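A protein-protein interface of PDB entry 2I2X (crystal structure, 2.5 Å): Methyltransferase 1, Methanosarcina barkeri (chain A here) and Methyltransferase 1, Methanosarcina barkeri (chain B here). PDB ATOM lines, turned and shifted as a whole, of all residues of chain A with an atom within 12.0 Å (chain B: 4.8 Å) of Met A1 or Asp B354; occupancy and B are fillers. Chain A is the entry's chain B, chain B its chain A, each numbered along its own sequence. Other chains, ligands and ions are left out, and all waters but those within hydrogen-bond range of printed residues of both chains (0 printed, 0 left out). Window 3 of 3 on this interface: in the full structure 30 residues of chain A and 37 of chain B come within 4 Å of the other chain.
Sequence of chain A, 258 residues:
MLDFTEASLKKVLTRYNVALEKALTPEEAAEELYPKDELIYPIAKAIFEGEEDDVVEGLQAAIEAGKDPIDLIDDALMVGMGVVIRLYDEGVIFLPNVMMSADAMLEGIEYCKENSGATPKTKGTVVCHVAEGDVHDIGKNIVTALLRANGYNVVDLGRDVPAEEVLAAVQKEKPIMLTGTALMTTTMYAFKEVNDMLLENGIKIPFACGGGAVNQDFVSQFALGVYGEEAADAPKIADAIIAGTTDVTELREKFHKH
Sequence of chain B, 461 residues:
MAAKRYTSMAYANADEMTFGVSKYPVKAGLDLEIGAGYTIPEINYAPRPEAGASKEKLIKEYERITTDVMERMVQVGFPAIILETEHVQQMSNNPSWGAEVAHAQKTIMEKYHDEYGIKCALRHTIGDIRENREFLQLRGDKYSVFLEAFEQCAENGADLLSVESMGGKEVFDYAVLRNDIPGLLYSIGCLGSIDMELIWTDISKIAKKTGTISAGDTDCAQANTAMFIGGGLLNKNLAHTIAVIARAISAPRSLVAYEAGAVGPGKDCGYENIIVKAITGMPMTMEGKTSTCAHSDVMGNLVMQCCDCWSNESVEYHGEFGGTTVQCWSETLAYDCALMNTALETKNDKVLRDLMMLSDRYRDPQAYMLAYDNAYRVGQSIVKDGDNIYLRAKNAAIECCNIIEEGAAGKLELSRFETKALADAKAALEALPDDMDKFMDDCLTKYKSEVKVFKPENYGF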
ATOM      1  N   MET A   1     -16.471 -21.401  21.921  1.00  0.00           N
ATOM      2  CA  MET A   1     -15.188 -20.715  22.261  1.00  0.00           C
ATOM      3  C   MET A   1     -15.232 -20.095  23.653  1.00  0.00           C
ATOM      4  O   MET A   1     -16.319 -19.776  24.161  1.00  0.00           O
ATOM      5  CB  MET A   1     -14.916 -19.608  21.238  1.00  0.00           C
ATOM      6  CG  MET A   1     -15.825 -18.428  21.346  1.00  0.00           C
ATOM      7  SD  MET A   1     -15.034 -16.968  20.641  1.00  0.00           S
ATOM      8  CE  MET A   1     -14.935 -17.475  18.949  1.00  0.00           C
ATOM      9  N   LEU A   2     -14.064 -19.843  24.228  1.00  0.00           N
ATOM     10  CA  LEU A   2     -13.985 -19.262  25.569  1.00  0.00           C
ATOM     11  C   LEU A   2     -14.458 -17.829  25.692  1.00  0.00           C
ATOM     12  O   LEU A   2     -14.302 -17.012  24.774  1.00  0.00           O
ATOM     13  CB  LEU A   2     -12.572 -19.367  26.132  1.00  0.00           C
ATOM     14  CG  LEU A   2     -12.034 -20.775  26.031  1.00  0.00           C
ATOM     15  CD1 LEU A   2     -10.576 -20.735  26.424  1.00  0.00           C
ATOM     16  CD2 LEU A   2     -12.849 -21.693  26.887  1.00  0.00           C
ATOM     17  N   ASP A   3     -15.036 -17.529  26.850  1.00  0.00           N
ATOM     18  CA  ASP A   3     -15.366 -16.152  27.211  1.00  0.00           C
ATOM     19  C   ASP A   3     -15.105 -15.966  28.707  1.00  0.00           C
ATOM     20  O   ASP A   3     -15.044 -16.918  29.449  1.00  0.00           O
ATOM     21  CB  ASP A   3     -16.818 -15.817  26.848  1.00  0.00           C
ATOM     22  CG  ASP A   3     -17.091 -14.307  26.861  1.00  0.00           C
ATOM     23  OD1 ASP A   3     -18.259 -13.911  27.083  1.00  0.00           O
ATOM     24  OD2 ASP A   3     -16.150 -13.499  26.666  1.00  0.00           O
ATOM     25  N   PHE A   4     -14.929 -14.727  29.122  1.00  0.00           N
ATOM     26  CA  PHE A   4     -14.787 -14.362  30.518  1.00  0.00           C
ATOM     27  C   PHE A   4     -16.136 -14.182  31.226  1.00  0.00           C
ATOM     28  O   PHE A   4     -17.126 -13.839  30.582  1.00  0.00           O
ATOM     29  CB  PHE A   4     -14.070 -13.015  30.580  1.00  0.00           C
ATOM     30  CG  PHE A   4     -12.587 -13.101  30.415  1.00  0.00           C
ATOM     31  CD1 PHE A   4     -11.904 -12.110  29.767  1.00  0.00           C
ATOM     32  CD2 PHE A   4     -11.867 -14.169  30.937  1.00  0.00           C
ATOM     33  CE1 PHE A   4     -10.532 -12.170  29.631  1.00  0.00           C
ATOM     34  CE2 PHE A   4     -10.501 -14.220  30.794  1.00  0.00           C
ATOM     35  CZ  PHE A   4      -9.841 -13.205  30.146  1.00  0.00           C
ATOM     36  N   THR A   5     -16.175 -14.407  32.542  1.00  0.00           N
ATOM     37  CA  THR A   5     -17.207 -13.808  33.393  1.00  0.00           C
ATOM     38  C   THR A   5     -16.832 -12.332  33.596  1.00  0.00           C
ATOM     39  O   THR A   5     -15.702 -11.943  33.336  1.00  0.00           O
ATOM     40  CB  THR A   5     -17.296 -14.472  34.791  1.00  0.00           C
ATOM     41  OG1 THR A   5     -16.107 -14.180  35.525  1.00  0.00           O
ATOM     42  CG2 THR A   5     -17.481 -15.959  34.701  1.00  0.00           C
ATOM     43  N   VAL A  12      -8.273  -9.312  34.655  1.00  0.00           N
ATOM     44  CA  VAL A  12      -7.249  -9.537  33.632  1.00  0.00           C
ATOM     45  C   VAL A  12      -6.722  -8.258  32.962  1.00  0.00           C
ATOM     46  O   VAL A  12      -5.547  -8.175  32.639  1.00  0.00           O
ATOM     47  CB  VAL A  12      -7.750 -10.569  32.583  1.00  0.00           C
ATOM     48  CG1 VAL A  12      -6.830 -10.613  31.364  1.00  0.00           C
ATOM     49  CG2 VAL A  12      -7.899 -11.967  33.223  1.00  0.00           C
ATOM     50  N   LEU A  13      -7.580  -7.266  32.737  1.00  0.00           N
ATOM     51  CA  LEU A  13      -7.101  -6.017  32.188  1.00  0.00           C
ATOM     52  C   LEU A  13      -7.921  -4.849  32.773  1.00  0.00           C
ATOM     53  O   LEU A  13      -8.917  -5.071  33.470  1.00  0.00           O
ATOM     54  CB  LEU A  13      -7.169  -6.067  30.646  1.00  0.00           C
ATOM     55  CG  LEU A  13      -8.553  -6.261  30.019  1.00  0.00           C
ATOM     56  CD1 LEU A  13      -9.362  -4.927  29.839  1.00  0.00           C
ATOM     57  CD2 LEU A  13      -8.490  -6.994  28.686  1.00  0.00           C
ATOM     58  N   LYS B 350      -6.665 -25.508  19.503  1.00  0.00           N
ATOM     59  CA  LYS B 350      -7.875 -24.691  19.521  1.00  0.00           C
ATOM     60  C   LYS B 350      -8.125 -23.977  20.833  1.00  0.00           C
ATOM     61  O   LYS B 350      -8.563 -22.825  20.815  1.00  0.00           O
ATOM     62  CB  LYS B 350      -9.094 -25.464  19.046  1.00  0.00           C
ATOM     63  CG  LYS B 350      -9.100 -25.631  17.516  1.00  0.00           C
ATOM     64  CD  LYS B 350     -10.350 -26.343  17.072  1.00  0.00           C
ATOM     65  CE  LYS B 350     -10.401 -26.468  15.574  1.00  0.00           C
ATOM     66  NZ  LYS B 350     -11.745 -27.062  15.253  1.00  0.00           N
ATOM     67  N   VAL B 351      -7.813 -24.628  21.958  1.00  0.00           N
ATOM     68  CA  VAL B 351      -8.003 -24.009  23.264  1.00  0.00           C
ATOM     69  C   VAL B 351      -6.980 -22.887  23.448  1.00  0.00           C
ATOM     70  O   VAL B 351      -7.280 -21.847  24.030  1.00  0.00           O
ATOM     71  CB  VAL B 351      -7.917 -25.036  24.450  1.00  0.00           C
ATOM     72  CG1 VAL B 351      -6.569 -25.688  24.491  1.00  0.00           C
ATOM     73  CG2 VAL B 351      -8.162 -24.355  25.817  1.00  0.00           C
ATOM     74  N   LEU B 352      -5.770 -23.101  22.945  1.00  0.00           N
ATOM     75  CA  LEU B 352      -4.724 -22.104  23.086  1.00  0.00           C
ATOM     76  C   LEU B 352      -5.078 -20.922  22.211  1.00  0.00           C
ATOM     77  O   LEU B 352      -5.032 -19.772  22.672  1.00  0.00           O
ATOM     78  CB  LEU B 352      -3.328 -22.683  22.774  1.00  0.00           C
ATOM     79  CG  LEU B 352      -2.159 -21.685  22.861  1.00  0.00           C
ATOM     80  CD1 LEU B 352      -2.089 -21.053  24.255  1.00  0.00           C
ATOM     81  CD2 LEU B 352      -0.845 -22.321  22.456  1.00  0.00           C
ATOM     82  N   ARG B 353      -5.461 -21.199  20.964  1.00  0.00           N
ATOM     83  CA  ARG B 353      -6.098 -20.183  20.118  1.00  0.00           C
ATOM     84  C   ARG B 353      -7.176 -19.374  20.878  1.00  0.00           C
ATOM     85  O   ARG B 353      -7.084 -18.153  20.972  1.00  0.00           O
ATOM     86  CB  ARG B 353      -6.609 -20.819  18.841  1.00  0.00           C
ATOM     87  CG  ARG B 353      -7.609 -19.986  17.967  1.00  0.00           C
ATOM     88  CD  ARG B 353      -8.989 -20.536  18.264  1.00  0.00           C
ATOM     89  NE  ARG B 353      -9.514 -21.292  17.163  1.00  0.00           N
ATOM     90  CZ  ARG B 353     -10.518 -22.157  17.217  1.00  0.00           C
ATOM     91  NH1 ARG B 353     -11.129 -22.444  18.357  1.00  0.00           N
ATOM     92  NH2 ARG B 353     -10.908 -22.722  16.067  1.00  0.00           N
ATOM     93  N   ASP B 354      -8.137 -20.028  21.512  1.00  0.00           N
ATOM     94  CA  ASP B 354      -9.113 -19.263  22.294  1.00  0.00           C
ATOM     95  C   ASP B 354      -8.515 -18.424  23.418  1.00  0.00           C
ATOM     96  O   ASP B 354      -8.964 -17.300  23.659  1.00  0.00           O
ATOM     97  CB  ASP B 354     -10.243 -20.147  22.798  1.00  0.00           C
ATOM     98  CG  ASP B 354     -11.108 -20.674  21.664  1.00  0.00           C
ATOM     99  OD1 ASP B 354     -11.009 -20.193  20.494  1.00  0.00           O
ATOM    100  OD2 ASP B 354     -11.909 -21.577  21.937  1.00  0.00           O
ATOM    101  N   LEU B 355      -7.490 -18.961  24.089  1.00  0.00           N
ATOM    102  CA  LEU B 355      -6.874 -18.288  25.222  1.00  0.00           C
ATOM    103  C   LEU B 355      -6.196 -16.994  24.712  1.00  0.00           C
ATOM    104  O   LEU B 355      -6.398 -15.906  25.259  1.00  0.00           O
ATOM    105  CB  LEU B 355      -5.874 -19.226  25.904  1.00  0.00           C
ATOM    106  CG  LEU B 355      -6.034 -19.909  27.277  1.00  0.00           C
ATOM    107  CD1 LEU B 355      -7.412 -19.910  27.871  1.00  0.00           C
ATOM    108  CD2 LEU B 355      -5.505 -21.315  27.216  1.00  0.00           C
ATOM    109  N   MET B 356      -5.449 -17.114  23.621  1.00  0.00           N
ATOM    110  CA  MET B 356      -4.782 -15.958  23.013  1.00  0.00           C
ATOM    111  C   MET B 356      -5.813 -14.920  22.624  1.00  0.00           C
ATOM    112  O   MET B 356      -5.625 -13.740  22.880  1.00  0.00           O
ATOM    113  CB  MET B 356      -3.951 -16.367  21.785  1.00  0.00           C
ATOM    114  CG  MET B 356      -2.978 -17.447  22.096  1.00  0.00           C
ATOM    115  SD  MET B 356      -2.075 -18.102  20.702  1.00  0.00           S
ATOM    116  CE  MET B 356      -3.382 -18.380  19.592  1.00  0.00           C
ATOM    117  N   MET B 357      -6.922 -15.375  22.050  1.00  0.00           N
ATOM    118  CA  MET B 357      -7.948 -14.472  21.581  1.00  0.00           C
ATOM    119  C   MET B 357      -8.560 -13.779  22.793  1.00  0.00           C
ATOM    120  O   MET B 357      -8.608 -12.546  22.845  1.00  0.00           O
ATOM    121  CB  MET B 357      -8.992 -15.227  20.730  1.00  0.00           C
ATOM    122  CG  MET B 357     -10.193 -14.408  20.272  1.00  0.00           C
ATOM    123  SD  MET B 357     -11.425 -14.034  21.563  1.00  0.00           S
ATOM    124  CE  MET B 357     -12.036 -15.689  21.968  1.00  0.00           C
ATOM    125  N   LEU B 358      -9.032 -14.561  23.752  1.00  0.00           N
ATOM    126  CA  LEU B 358      -9.758 -14.011  24.924  1.00  0.00           C
ATOM    127  C   LEU B 358      -8.927 -13.000  25.751  1.00  0.00           C
ATOM    128  O   LEU B 358      -9.473 -12.013  26.306  1.00  0.00           O
ATOM    129  CB  LEU B 358     -10.314 -15.138  25.827  1.00  0.00           C
ATOM    130  CG  LEU B 358     -11.161 -14.687  27.019  1.00  0.00           C
ATOM    131  CD1 LEU B 358     -12.350 -13.819  26.561  1.00  0.00           C
ATOM    132  CD2 LEU B 358     -11.657 -15.885  27.850  1.00  0.00           C
ATOM    133  N   SER B 359      -7.626 -13.265  25.826  1.00  0.00           N
ATOM    134  CA  SER B 359      -6.633 -12.355  26.424  1.00  0.00           C
ATOM    135  C   SER B 359      -6.877 -10.880  26.085  1.00  0.00           C
ATOM    136  O   SER B 359      -6.828  -9.990  26.951  1.00  0.00           O
ATOM    137  CB  SER B 359      -5.241 -12.758  25.922  1.00  0.00           C
ATOM    138  OG  SER B 359      -4.271 -11.752  26.202  1.00  0.00           O
ATOM    139  N   ARG B 361      -9.476  -9.767  23.669  1.00  0.00           N
ATOM    140  CA  ARG B 361     -10.794  -9.436  23.142  1.00  0.00           C
ATOM    141  C   ARG B 361     -11.386  -8.144  23.745  1.00  0.00           C
ATOM    142  O   ARG B 361     -12.068  -7.386  23.017  1.00  0.00           O
ATOM    143  CB  ARG B 361     -11.816 -10.622  23.245  1.00  0.00           C
ATOM    144  CG  ARG B 361     -13.306 -10.169  23.034  1.00  0.00           C
ATOM    145  CD  ARG B 361     -14.394 -11.278  23.113  1.00  0.00           C
ATOM    146  NE  ARG B 361     -14.178 -12.080  21.950  1.00  0.00           N
ATOM    147  CZ  ARG B 361     -15.020 -12.329  20.963  1.00  0.00           C
ATOM    148  NH1 ARG B 361     -16.273 -11.903  20.970  1.00  0.00           N
ATOM    149  NH2 ARG B 361     -14.557 -13.077  19.969  1.00  0.00           N
ATOM    150  N   TYR B 372     -10.878 -13.807  15.998  1.00  0.00           N
ATOM    151  CA  TYR B 372     -11.076 -14.611  14.800  1.00  0.00           C
ATOM    152  C   TYR B 372     -12.555 -14.856  14.481  1.00  0.00           C
ATOM    153  O   TYR B 372     -12.909 -14.941  13.306  1.00  0.00           O
ATOM    154  CB  TYR B 372     -10.270 -15.926  14.849  1.00  0.00           C
ATOM    155  CG  TYR B 372     -10.843 -16.943  15.816  1.00  0.00           C
ATOM    156  CD1 TYR B 372     -10.477 -16.929  17.166  1.00  0.00           C
ATOM    157  CD2 TYR B 372     -11.801 -17.896  15.387  1.00  0.00           C
ATOM    158  CE1 TYR B 372     -11.036 -17.850  18.065  1.00  0.00           C
ATOM    159  CE2 TYR B 372     -12.372 -18.811  16.279  1.00  0.00           C
ATOM    160  CZ  TYR B 372     -11.986 -18.789  17.618  1.00  0.00           C
ATOM    161  OH  TYR B 372     -12.552 -19.690  18.515  1.00  0.00           O
ATOM    162  N   ASP B 373     -13.423 -14.967  15.479  1.00  0.00           N
ATOM    163  CA  ASP B 373     -14.856 -15.085  15.155  1.00  0.00           C
ATOM    164  C   ASP B 373     -15.422 -13.822  14.501  1.00  0.00           C
ATOM    165  O   ASP B 373     -16.200 -13.920  13.544  1.00  0.00           O
ATOM    166  CB  ASP B 373     -15.720 -15.502  16.346  1.00  0.00           C
ATOM    167  CG  ASP B 373     -15.604 -14.546  17.488  1.00  0.00           C
ATOM    168  OD1 ASP B 373     -14.489 -13.990  17.633  1.00  0.00           O
ATOM    169  OD2 ASP B 373     -16.597 -14.336  18.244  1.00  0.00           O
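Along chain A the printed residues that touch a printed residue of chain B span positions 1 to 13.
Printed residues of chain B that touch a printed residue of chain A: Asp B354, Leu B355, Met B357, Leu B358, Ser B359, Arg B361, Tyr B372 and Asp B373.
The guanidinium group (NH1) of Arg B353 lies within salt-bridge range of the side-chain carboxylate (OD1) of Asp B354 (3.1 Å).
OH of Tyr B372 sits at hydrogen-bond distance from NH1 of Arg B353 (3.1 Å).
The side-chain hydroxyl (OH) of Tyr B372 sits at hydrogen-bond distance from the side-chain carboxylate (OD1) of Asp B354, at 2.6 Å.
SD of Met B357 sits at hydrogen-bond distance from NE of Arg B361, at 3.4 Å.
The guanidinium group (NH2) of Arg B361 lies within salt-bridge range of the side-chain carboxylate (OD1) of Asp B373.
Asp B354 touches Met A1 (OD2 to CA, 3.4 Å).
Met A1 touches Met B357 (SD to CE, 3.5 Å).
SD of Met A1 touches NH2 of Arg B361, at 3.98 Å.
Tyr B372 touches Met A1 (OH to CE, 3.3 Å).
CE of Met A1 touches CG of Asp B373 (3.3 Å).
N of Leu A2 touches OD2 of Asp B354 (3.6 Å).
CD1 of Leu A2 touches CD1 of Leu B355, at 3.6 Å.
C of Asp A3 touches CD2 of Leu B358, at 3.6 Å.
O of Leu B358 touches CE1 of Phe A4 (3.5 Å).
Ser B359 touches Leu A13.
Printed residues of chain B within 4 Å of Met A1: Asp B354, Met B357, Arg B361, Tyr B372 and Asp B373.
Asp B354 touches just these residues of chain A: Met A1 (3.4 Å) and Leu A2 (3.6 Å).
No residue of chain A comes within 4 Å of Val B351.
No residue of chain A comes within 4 Å of Arg B353.
Of chain A, only Leu A2 comes within 4 Å of Leu B355.
Asp B373 touches just one residue of chain A: Met A1 (3.3 Å).
Of the printed residues of chain A, Leu B358 touches Leu A2 (3.99 Å), Asp A3 (3.6 Å) and Phe A4 (3.5 Å).
Of the printed residues of chain A, Arg B361 touches Met A1 (3.98 Å).
Printed residues of chain B within 4 Å of Phe A4: Leu B358 (3.5 Å).
Printed residues of chain B within 4 Å of Leu A2: Asp B354 (3.6 Å), Leu B355 (3.6 Å), Met B357 (3.8 Å) and Leu B358 (3.99 Å).
The nearest printed residue of chain B that does not touch Asp A3 is Arg B361 (4.5 Å).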
